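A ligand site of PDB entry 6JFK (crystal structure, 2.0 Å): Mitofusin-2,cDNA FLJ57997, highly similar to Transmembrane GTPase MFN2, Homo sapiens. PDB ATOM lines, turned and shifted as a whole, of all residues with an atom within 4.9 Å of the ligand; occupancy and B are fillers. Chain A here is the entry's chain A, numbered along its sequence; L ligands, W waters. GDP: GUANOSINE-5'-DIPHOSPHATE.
Thr 91 touches the ligand (C to O3B, 3.8 Å). Gly 111 touches the ligand (C to O3', 3.5 Å). Hydrophobic or aromatic side chains within 4 Å of the ligand: Ile 112. Of the 23 residues printed, 16 come within 4 Å of the ligand.
An oxygen (O1A) of the ligand lies within hydrogen-bond range of the backbone NH (N) of Thr 97 (2.8 Å). The side-chain hydroxyl (OG1) of Thr 97 lies within hydrogen-bond range of an oxygen (O1A) of the ligand, at 2.6 Å. The side-chain carboxylate of Asp 247 is in hydrogen-bond range of a nitrogen (N1) of the ligand. N of Lys 95 sits at hydrogen-bond distance from O1B of the ligand. An oxygen (O1B) of the ligand sits at hydrogen-bond distance from the backbone NH (N) of Gly 94 (2.8 Å). O3B of the ligand is in hydrogen-bond range of N of Ser 92, 2.8 Å away. The backbone NH (N) of Ser 96 lies within hydrogen-bond range of an oxygen (O2B) of the ligand (3.0 Å). The side-chain hydroxyl (OG) of Ser 96 is in hydrogen-bond range of an oxygen (O2B) of the ligand (3.0 Å). An oxygen (O6) of the ligand sits at hydrogen-bond distance from the backbone NH (N) of Ala 292 (3.1 Å). The backbone NH (N) of Arg 245 sits at hydrogen-bond distance from an oxygen (O6) of the ligand (3.3 Å). NH1 of Arg 245 lies within hydrogen-bond range of O4' of the ligand (3.1 Å). The side-chain amide oxygen (OD1) of Asn 244 sits close to a nitrogen (N7) of the ligand, 3.1 Å away. An oxygen (O2') of the ligand lies close to the backbone carbonyl oxygen (O) of Ser 110, at 3.5 Å. An oxygen (O6) of the ligand sits at hydrogen-bond distance from the side-chain hydroxyl of Ser 291, 3.2 Å away. An oxygen (O3') of the ligand lies close to the backbone NH (N) of Ile 112 (3.3 Å). The backbone NH of Asn 93 sits at hydrogen-bond distance from an oxygen (O1B) of the ligand (3.4 Å). An oxygen (O2') of the ligand sits at hydrogen-bond distance from the side-chain amino group (NZ) of Lys 293, at 3.4 Å.
Water W4 bridges an oxygen (O2A) of the ligand (2.7 Å) and the backbone carbonyl oxygen of Gly 111 (2.8 Å). Water W5 lies within hydrogen-bond range of an oxygen (O3B) of the ligand and the side-chain amino group (NZ) of Lys 95. Water W3 lies within hydrogen-bond range of an oxygen (O2A) of the ligand (2.7 Å), the side-chain hydroxyl of Ser 96 (2.9 Å) and the backbone carbonyl oxygen of Pro 109 (3.3 Å). Water W6 lies within hydrogen-bond range of OG1 of Thr 97, O of Ser 110 and O2' of the ligand. Water W7 lies within hydrogen-bond range of the side-chain hydroxyl of Thr 116 (2.6 Å), the side-chain hydroxyl of Ser 96 (2.8 Å), an oxygen (O2B) of the ligand (2.9 Å) and the side-chain carboxylate of Asp 185 (2.9 Å). Water W1 bridges N3 of the ligand and NZ of Lys 293.
OD1 of Asp 247 is in hydrogen-bond range of OG of Ser 291 (2.7 Å). The guanidinium group (NH1) of Arg 245 lies within hydrogen-bond range of the backbone carbonyl oxygen (O) of Ser 92. The side-chain carboxylate (OD2) of Asp 185 lies within hydrogen-bond range of the side-chain hydroxyl (OG) of Ser 96 (2.5 Å). The backbone NH (N) of Ala 292 sits close to the side-chain amide nitrogen (ND2) of Asn 244 (2.8 Å). The backbone NH (N) of Arg 245 is in hydrogen-bond range of the backbone carbonyl oxygen (O) of Val 290 (3.2 Å). The backbone carbonyl oxygen (O) of Asn 93 lies close to the side-chain amide oxygen (OD1) of Asn 244 (2.8 Å). The side-chain amide nitrogen of Asn 93 sits close to the backbone NH of Arg 90 (3.3 Å).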
ATOM      1  N   ARG A  90      -9.807   4.308 -21.105  1.00  0.00           N
ATOM      2  CA  ARG A  90      -8.584   5.098 -21.027  1.00  0.00           C
ATOM      3  C   ARG A  90      -7.444   4.232 -20.496  1.00  0.00           C
ATOM      4  O   ARG A  90      -7.661   3.329 -19.682  1.00  0.00           O
ATOM      5  CB  ARG A  90      -8.787   6.331 -20.122  1.00  0.00           C
ATOM      6  CG  ARG A  90      -7.495   7.025 -19.642  1.00  0.00           C
ATOM      7  CD  ARG A  90      -7.778   8.443 -19.112  1.00  0.00           C
ATOM      8  NE  ARG A  90      -8.242   9.361 -20.164  1.00  0.00           N
ATOM      9  CZ  ARG A  90      -8.522  10.650 -19.966  1.00  0.00           C
ATOM     10  NH1 ARG A  90      -8.361  11.193 -18.771  1.00  0.00           N
ATOM     11  NH2 ARG A  90      -8.954  11.392 -20.974  1.00  0.00           N
ATOM     12  N   THR A  91      -6.226   4.526 -20.967  1.00  0.00           N
ATOM     13  CA  THR A  91      -5.029   3.802 -20.530  1.00  0.00           C
ATOM     14  C   THR A  91      -4.987   3.696 -19.015  1.00  0.00           C
ATOM     15  O   THR A  91      -5.273   4.664 -18.316  1.00  0.00           O
ATOM     16  CB  THR A  91      -3.766   4.518 -21.037  1.00  0.00           C
ATOM     17  OG1 THR A  91      -3.704   4.429 -22.471  1.00  0.00           O
ATOM     18  CG2 THR A  91      -2.511   3.886 -20.451  1.00  0.00           C
ATOM     19  N   SER A  92      -4.632   2.503 -18.512  1.00  0.00           N
ATOM     20  CA  SER A  92      -4.408   2.221 -17.097  1.00  0.00           C
ATOM     21  C   SER A  92      -5.685   2.147 -16.276  1.00  0.00           C
ATOM     22  O   SER A  92      -5.604   2.053 -15.038  1.00  0.00           O
ATOM     23  CB  SER A  92      -3.456   3.248 -16.449  1.00  0.00           C
ATOM     24  OG  SER A  92      -2.414   2.605 -15.740  1.00  0.00           O
ATOM     25  N   ASN A  93      -6.861   2.171 -16.907  1.00  0.00           N
ATOM     26  CA  ASN A  93      -8.083   1.895 -16.165  1.00  0.00           C
ATOM     27  C   ASN A  93      -8.120   0.456 -15.673  1.00  0.00           C
ATOM     28  O   ASN A  93      -8.730   0.173 -14.628  1.00  0.00           O
ATOM     29  CB  ASN A  93      -9.314   2.144 -17.038  1.00  0.00           C
ATOM     30  CG  ASN A  93      -9.639   3.604 -17.210  1.00  0.00           C
ATOM     31  OD1 ASN A  93      -8.942   4.481 -16.703  1.00  0.00           O
ATOM     32  ND2 ASN A  93     -10.705   3.881 -17.963  1.00  0.00           N
ATOM     33  N   GLY A  94      -7.504  -0.482 -16.413  1.00  0.00           N
ATOM     34  CA  GLY A  94      -7.478  -1.878 -15.989  1.00  0.00           C
ATOM     35  C   GLY A  94      -7.989  -2.914 -16.987  1.00  0.00           C
ATOM     36  O   GLY A  94      -8.297  -4.049 -16.580  1.00  0.00           O
ATOM     37  N   LYS A  95      -8.059  -2.573 -18.279  1.00  0.00           N
ATOM     38  CA  LYS A  95      -8.614  -3.486 -19.284  1.00  0.00           C
ATOM     39  C   LYS A  95      -7.886  -4.830 -19.287  1.00  0.00           C
ATOM     40  O   LYS A  95      -8.513  -5.892 -19.223  1.00  0.00           O
ATOM     41  CB  LYS A  95      -8.524  -2.865 -20.690  1.00  0.00           C
ATOM     42  CG  LYS A  95      -9.432  -1.694 -20.965  1.00  0.00           C
ATOM     43  CD  LYS A  95      -9.219  -1.161 -22.390  1.00  0.00           C
ATOM     44  CE  LYS A  95      -7.818  -0.599 -22.554  1.00  0.00           C
ATOM     45  NZ  LYS A  95      -7.788   0.414 -23.629  1.00  0.00           N
ATOM     46  N   SER A  96      -6.563  -4.791 -19.394  1.00  0.00           N
ATOM     47  CA  SER A  96      -5.790  -6.040 -19.482  1.00  0.00           C
ATOM     48  C   SER A  96      -5.929  -6.862 -18.204  1.00  0.00           C
ATOM     49  O   SER A  96      -5.980  -8.088 -18.252  1.00  0.00           O
ATOM     50  CB  SER A  96      -4.321  -5.737 -19.767  1.00  0.00           C
ATOM     51  OG  SER A  96      -4.189  -4.987 -20.970  1.00  0.00           O
ATOM     52  N   THR A  97      -5.972  -6.190 -17.045  1.00  0.00           N
ATOM     53  CA  THR A  97      -6.162  -6.910 -15.784  1.00  0.00           C
ATOM     54  C   THR A  97      -7.531  -7.586 -15.737  1.00  0.00           C
ATOM     55  O   THR A  97      -7.646  -8.723 -15.262  1.00  0.00           O
ATOM     56  CB  THR A  97      -5.988  -5.945 -14.603  1.00  0.00           C
ATOM     57  OG1 THR A  97      -4.698  -5.300 -14.672  1.00  0.00           O
ATOM     58  CG2 THR A  97      -6.046  -6.707 -13.271  1.00  0.00           C
ATOM     59  N   PRO A 109       0.148  -8.552 -21.052  1.00  0.00           N
ATOM     60  CA  PRO A 109       0.943  -7.705 -20.169  1.00  0.00           C
ATOM     61  C   PRO A 109       0.028  -6.702 -19.486  1.00  0.00           C
ATOM     62  O   PRO A 109      -0.807  -6.079 -20.131  1.00  0.00           O
ATOM     63  CB  PRO A 109       1.926  -7.010 -21.125  1.00  0.00           C
ATOM     64  CG  PRO A 109       1.795  -7.704 -22.440  1.00  0.00           C
ATOM     65  CD  PRO A 109       0.430  -8.313 -22.478  1.00  0.00           C
ATOM     66  N   SER A 110       0.166  -6.592 -18.160  1.00  0.00           N
ATOM     67  CA  SER A 110      -0.722  -5.691 -17.414  1.00  0.00           C
ATOM     68  C   SER A 110      -0.058  -5.155 -16.145  1.00  0.00           C
ATOM     69  O   SER A 110      -0.765  -4.870 -15.164  1.00  0.00           O
ATOM     70  CB  SER A 110      -2.035  -6.393 -17.064  1.00  0.00           C
ATOM     71  OG  SER A 110      -1.856  -7.431 -16.099  1.00  0.00           O
ATOM     72  N   GLY A 111       1.261  -4.994 -16.151  1.00  0.00           N
ATOM     73  CA  GLY A 111       1.971  -4.509 -14.974  1.00  0.00           C
ATOM     74  C   GLY A 111       2.210  -3.005 -14.997  1.00  0.00           C
ATOM     75  O   GLY A 111       1.907  -2.313 -15.962  1.00  0.00           O
ATOM     76  N   ILE A 112       2.799  -2.510 -13.893  1.00  0.00           N
ATOM     77  CA  ILE A 112       3.152  -1.107 -13.801  1.00  0.00           C
ATOM     78  C   ILE A 112       4.221  -0.763 -14.833  1.00  0.00           C
ATOM     79  O   ILE A 112       5.146  -1.555 -15.108  1.00  0.00           O
ATOM     80  CB  ILE A 112       3.653  -0.720 -12.394  1.00  0.00           C
ATOM     81  CG1 ILE A 112       4.768  -1.695 -11.944  1.00  0.00           C
ATOM     82  CG2 ILE A 112       2.499  -0.655 -11.417  1.00  0.00           C
ATOM     83  CD1 ILE A 112       5.538  -1.217 -10.715  1.00  0.00           C
ATOM     84  N   THR A 116       0.150  -0.865 -23.611  1.00  0.00           N
ATOM     85  CA  THR A 116      -0.052  -1.599 -24.864  1.00  0.00           C
ATOM     86  C   THR A 116      -0.499  -0.636 -25.960  1.00  0.00           C
ATOM     87  O   THR A 116      -1.545   0.010 -25.827  1.00  0.00           O
ATOM     88  CB  THR A 116      -1.099  -2.701 -24.701  1.00  0.00           C
ATOM     89  OG1 THR A 116      -2.154  -2.245 -23.858  1.00  0.00           O
ATOM     90  CG2 THR A 116      -0.460  -3.956 -24.137  1.00  0.00           C
ATOM     91  N   ASP A 185      -8.480  -6.891 -26.431  1.00  0.00           N
ATOM     92  CA  ASP A 185      -7.934  -5.749 -25.706  1.00  0.00           C
ATOM     93  C   ASP A 185      -7.632  -4.644 -26.716  1.00  0.00           C
ATOM     94  O   ASP A 185      -7.361  -4.905 -27.894  1.00  0.00           O
ATOM     95  CB  ASP A 185      -6.667  -6.186 -24.967  1.00  0.00           C
ATOM     96  CG  ASP A 185      -6.210  -5.199 -23.882  1.00  0.00           C
ATOM     97  OD1 ASP A 185      -6.790  -4.117 -23.720  1.00  0.00           O
ATOM     98  OD2 ASP A 185      -5.238  -5.541 -23.184  1.00  0.00           O
ATOM     99  N   ASN A 244     -13.791   0.059 -12.423  1.00  0.00           N
ATOM    100  CA  ASN A 244     -12.654  -0.693 -11.919  1.00  0.00           C
ATOM    101  C   ASN A 244     -11.873   0.135 -10.914  1.00  0.00           C
ATOM    102  O   ASN A 244     -12.084   1.343 -10.762  1.00  0.00           O
ATOM    103  CB  ASN A 244     -11.760  -1.140 -13.083  1.00  0.00           C
ATOM    104  CG  ASN A 244     -10.702  -2.142 -12.664  1.00  0.00           C
ATOM    105  OD1 ASN A 244      -9.513  -1.992 -12.998  1.00  0.00           O
ATOM    106  ND2 ASN A 244     -11.105  -3.128 -11.875  1.00  0.00           N
ATOM    107  N   ARG A 245     -10.927  -0.527 -10.234  1.00  0.00           N
ATOM    108  CA  ARG A 245     -10.077   0.087  -9.218  1.00  0.00           C
ATOM    109  C   ARG A 245     -10.871   0.478  -7.979  1.00  0.00           C
ATOM    110  O   ARG A 245     -10.467   1.361  -7.203  1.00  0.00           O
ATOM    111  CB  ARG A 245      -9.303   1.308  -9.771  1.00  0.00           C
ATOM    112  CG  ARG A 245      -8.617   1.067 -11.124  1.00  0.00           C
ATOM    113  CD  ARG A 245      -7.911   2.324 -11.638  1.00  0.00           C
ATOM    114  NE  ARG A 245      -6.765   2.623 -10.785  1.00  0.00           N
ATOM    115  CZ  ARG A 245      -5.532   2.175 -10.982  1.00  0.00           C
ATOM    116  NH1 ARG A 245      -5.239   1.442 -12.042  1.00  0.00           N
ATOM    117  NH2 ARG A 245      -4.569   2.479 -10.115  1.00  0.00           N
ATOM    118  N   TRP A 246     -11.983  -0.226  -7.741  1.00  0.00           N
ATOM    119  CA  TRP A 246     -12.865   0.177  -6.660  1.00  0.00           C
ATOM    120  C   TRP A 246     -12.285  -0.151  -5.284  1.00  0.00           C
ATOM    121  O   TRP A 246     -12.809   0.334  -4.269  1.00  0.00           O
ATOM    122  CB  TRP A 246     -14.236  -0.478  -6.869  1.00  0.00           C
ATOM    123  CG  TRP A 246     -15.321  -0.001  -5.896  1.00  0.00           C
ATOM    124  CD1 TRP A 246     -16.069  -0.769  -5.057  1.00  0.00           C
ATOM    125  CD2 TRP A 246     -15.771   1.361  -5.705  1.00  0.00           C
ATOM    126  NE1 TRP A 246     -16.950   0.013  -4.354  1.00  0.00           N
ATOM    127  CE2 TRP A 246     -16.784   1.328  -4.722  1.00  0.00           C
ATOM    128  CE3 TRP A 246     -15.407   2.592  -6.255  1.00  0.00           C
ATOM    129  CZ2 TRP A 246     -17.437   2.492  -4.275  1.00  0.00           C
ATOM    130  CZ3 TRP A 246     -16.058   3.747  -5.813  1.00  0.00           C
ATOM    131  CH2 TRP A 246     -17.067   3.685  -4.839  1.00  0.00           C
ATOM    132  N   ASP A 247     -11.182  -0.918  -5.222  1.00  0.00           N
ATOM    133  CA  ASP A 247     -10.459  -1.063  -3.955  1.00  0.00           C
ATOM    134  C   ASP A 247      -9.994   0.283  -3.414  1.00  0.00           C
ATOM    135  O   ASP A 247      -9.833   0.448  -2.184  1.00  0.00           O
ATOM    136  CB  ASP A 247      -9.273  -2.005  -4.141  1.00  0.00           C
ATOM    137  CG  ASP A 247      -8.360  -1.606  -5.322  1.00  0.00           C
ATOM    138  OD1 ASP A 247      -8.761  -1.802  -6.493  1.00  0.00           O
ATOM    139  OD2 ASP A 247      -7.242  -1.111  -5.073  1.00  0.00           O
ATOM    140  N   VAL A 290     -15.735  -2.985  -9.146  1.00  0.00           N
ATOM    141  CA  VAL A 290     -14.859  -4.136  -8.985  1.00  0.00           C
ATOM    142  C   VAL A 290     -13.408  -3.698  -8.793  1.00  0.00           C
ATOM    143  O   VAL A 290     -13.044  -2.533  -9.013  1.00  0.00           O
ATOM    144  CB  VAL A 290     -14.943  -5.098 -10.194  1.00  0.00           C
ATOM    145  CG1 VAL A 290     -16.357  -5.684 -10.342  1.00  0.00           C
ATOM    146  CG2 VAL A 290     -14.473  -4.379 -11.457  1.00  0.00           C
ATOM    147  N   SER A 291     -12.574  -4.661  -8.400  1.00  0.00           N
ATOM    148  CA  SER A 291     -11.121  -4.500  -8.361  1.00  0.00           C
ATOM    149  C   SER A 291     -10.541  -5.665  -9.156  1.00  0.00           C
ATOM    150  O   SER A 291     -10.356  -6.766  -8.609  1.00  0.00           O
ATOM    151  CB  SER A 291     -10.579  -4.479  -6.933  1.00  0.00           C
ATOM    152  OG  SER A 291      -9.161  -4.417  -6.976  1.00  0.00           O
ATOM    153  N   ALA A 292     -10.272  -5.429 -10.443  1.00  0.00           N
ATOM    154  CA  ALA A 292      -9.801  -6.513 -11.299  1.00  0.00           C
ATOM    155  C   ALA A 292      -8.466  -7.059 -10.825  1.00  0.00           C
ATOM    156  O   ALA A 292      -8.173  -8.240 -11.007  1.00  0.00           O
ATOM    157  CB  ALA A 292      -9.678  -6.037 -12.749  1.00  0.00           C
ATOM    158  N   LYS A 293      -7.647  -6.203 -10.185  1.00  0.00           N
ATOM    159  CA  LYS A 293      -6.353  -6.661  -9.697  1.00  0.00           C
ATOM    160  C   LYS A 293      -6.522  -7.614  -8.527  1.00  0.00           C
ATOM    161  O   LYS A 293      -5.788  -8.598  -8.407  1.00  0.00           O
ATOM    162  CB  LYS A 293      -5.470  -5.472  -9.299  1.00  0.00           C
ATOM    163  CG  LYS A 293      -4.094  -5.919  -8.859  1.00  0.00           C
ATOM    164  CD  LYS A 293      -3.167  -4.752  -8.577  1.00  0.00           C
ATOM    165  CE  LYS A 293      -1.712  -5.195  -8.741  1.00  0.00           C
ATOM    166  NZ  LYS A 293      -0.774  -4.037  -8.783  1.00  0.00           N
ATOM    167  N   LEU A 313      -6.641  -6.322  -1.592  1.00  0.00           N
ATOM    168  CA  LEU A 313      -5.895  -5.065  -1.535  1.00  0.00           C
ATOM    169  C   LEU A 313      -6.383  -4.128  -0.448  1.00  0.00           C
ATOM    170  O   LEU A 313      -5.656  -3.214  -0.063  1.00  0.00           O
ATOM    171  CB  LEU A 313      -5.965  -4.339  -2.891  1.00  0.00           C
ATOM    172  CG  LEU A 313      -5.330  -5.133  -4.036  1.00  0.00           C
ATOM    173  CD1 LEU A 313      -5.635  -4.487  -5.393  1.00  0.00           C
ATOM    174  CD2 LEU A 313      -3.837  -5.254  -3.792  1.00  0.00           C
HETATM  175  PB  GDP L   1      -5.004  -0.966 -19.096  1.00  0.00           P
HETATM  176  O1B GDP L   1      -6.409  -0.448 -18.964  1.00  0.00           O
HETATM  177  O2B GDP L   1      -4.950  -2.300 -19.872  1.00  0.00           O
HETATM  178  O3B GDP L   1      -4.107   0.036 -19.780  1.00  0.00           O
HETATM  179  O3A GDP L   1      -4.521  -1.210 -17.577  1.00  0.00           O
HETATM  180  PA  GDP L   1      -3.870  -2.511 -16.911  1.00  0.00           P
HETATM  181  O1A GDP L   1      -4.819  -3.674 -16.747  1.00  0.00           O
HETATM  182  O2A GDP L   1      -2.554  -2.821 -17.542  1.00  0.00           O
HETATM  183  O5' GDP L   1      -3.579  -1.930 -15.430  1.00  0.00           O
HETATM  184  C5' GDP L   1      -2.703  -0.797 -15.248  1.00  0.00           C
HETATM  185  C4' GDP L   1      -2.111  -0.808 -13.838  1.00  0.00           C
HETATM  186  O4' GDP L   1      -3.203  -0.716 -12.929  1.00  0.00           O
HETATM  187  C3' GDP L   1      -1.413  -2.128 -13.555  1.00  0.00           C
HETATM  188  O3' GDP L   1      -0.276  -1.902 -12.732  1.00  0.00           O
HETATM  189  C2' GDP L   1      -2.459  -2.933 -12.805  1.00  0.00           C
HETATM  190  O2' GDP L   1      -1.866  -3.948 -11.997  1.00  0.00           O
HETATM  191  C1' GDP L   1      -3.209  -1.855 -12.057  1.00  0.00           C
HETATM  192  N9  GDP L   1      -4.617  -2.238 -11.826  1.00  0.00           N
HETATM  193  C8  GDP L   1      -5.476  -2.806 -12.700  1.00  0.00           C
HETATM  194  N7  GDP L   1      -6.688  -3.002 -12.143  1.00  0.00           N
HETATM  195  C5  GDP L   1      -6.620  -2.546 -10.884  1.00  0.00           C
HETATM  196  C6  GDP L   1      -7.525  -2.443  -9.730  1.00  0.00           C
HETATM  197  O6  GDP L   1      -8.701  -2.866  -9.791  1.00  0.00           O
HETATM  198  N1  GDP L   1      -7.046  -1.897  -8.598  1.00  0.00           N
HETATM  199  C2  GDP L   1      -5.789  -1.435  -8.469  1.00  0.00           C
HETATM  200  N2  GDP L   1      -5.393  -0.898  -7.273  1.00  0.00           N
HETATM  201  N3  GDP L   1      -4.895  -1.505  -9.482  1.00  0.00           N
HETATM  202  C4  GDP L   1      -5.256  -2.034 -10.688  1.00  0.00           C
HETATM  203  O   HOH W   1      -2.005  -0.935  -8.745  1.00  0.00           O
HETATM  204  O   HOH W   2      -0.608  -0.218 -10.663  1.00  0.00           O
HETATM  205  O   HOH W   3      -2.150  -3.023 -20.231  1.00  0.00           O
HETATM  206  O   HOH W   4      -0.085  -1.845 -17.844  1.00  0.00           O
HETATM  207  O   HOH W   5      -4.898   0.554 -22.290  1.00  0.00           O
HETATM  208  O   HOH W   6      -2.401  -6.424 -13.401  1.00  0.00           O
HETATM  209  O   HOH W   7      -4.376  -2.766 -22.707  1.00  0.00           O
HETATM  210  O   HOH W   8      -1.441   0.253 -19.235  1.00  0.00           O
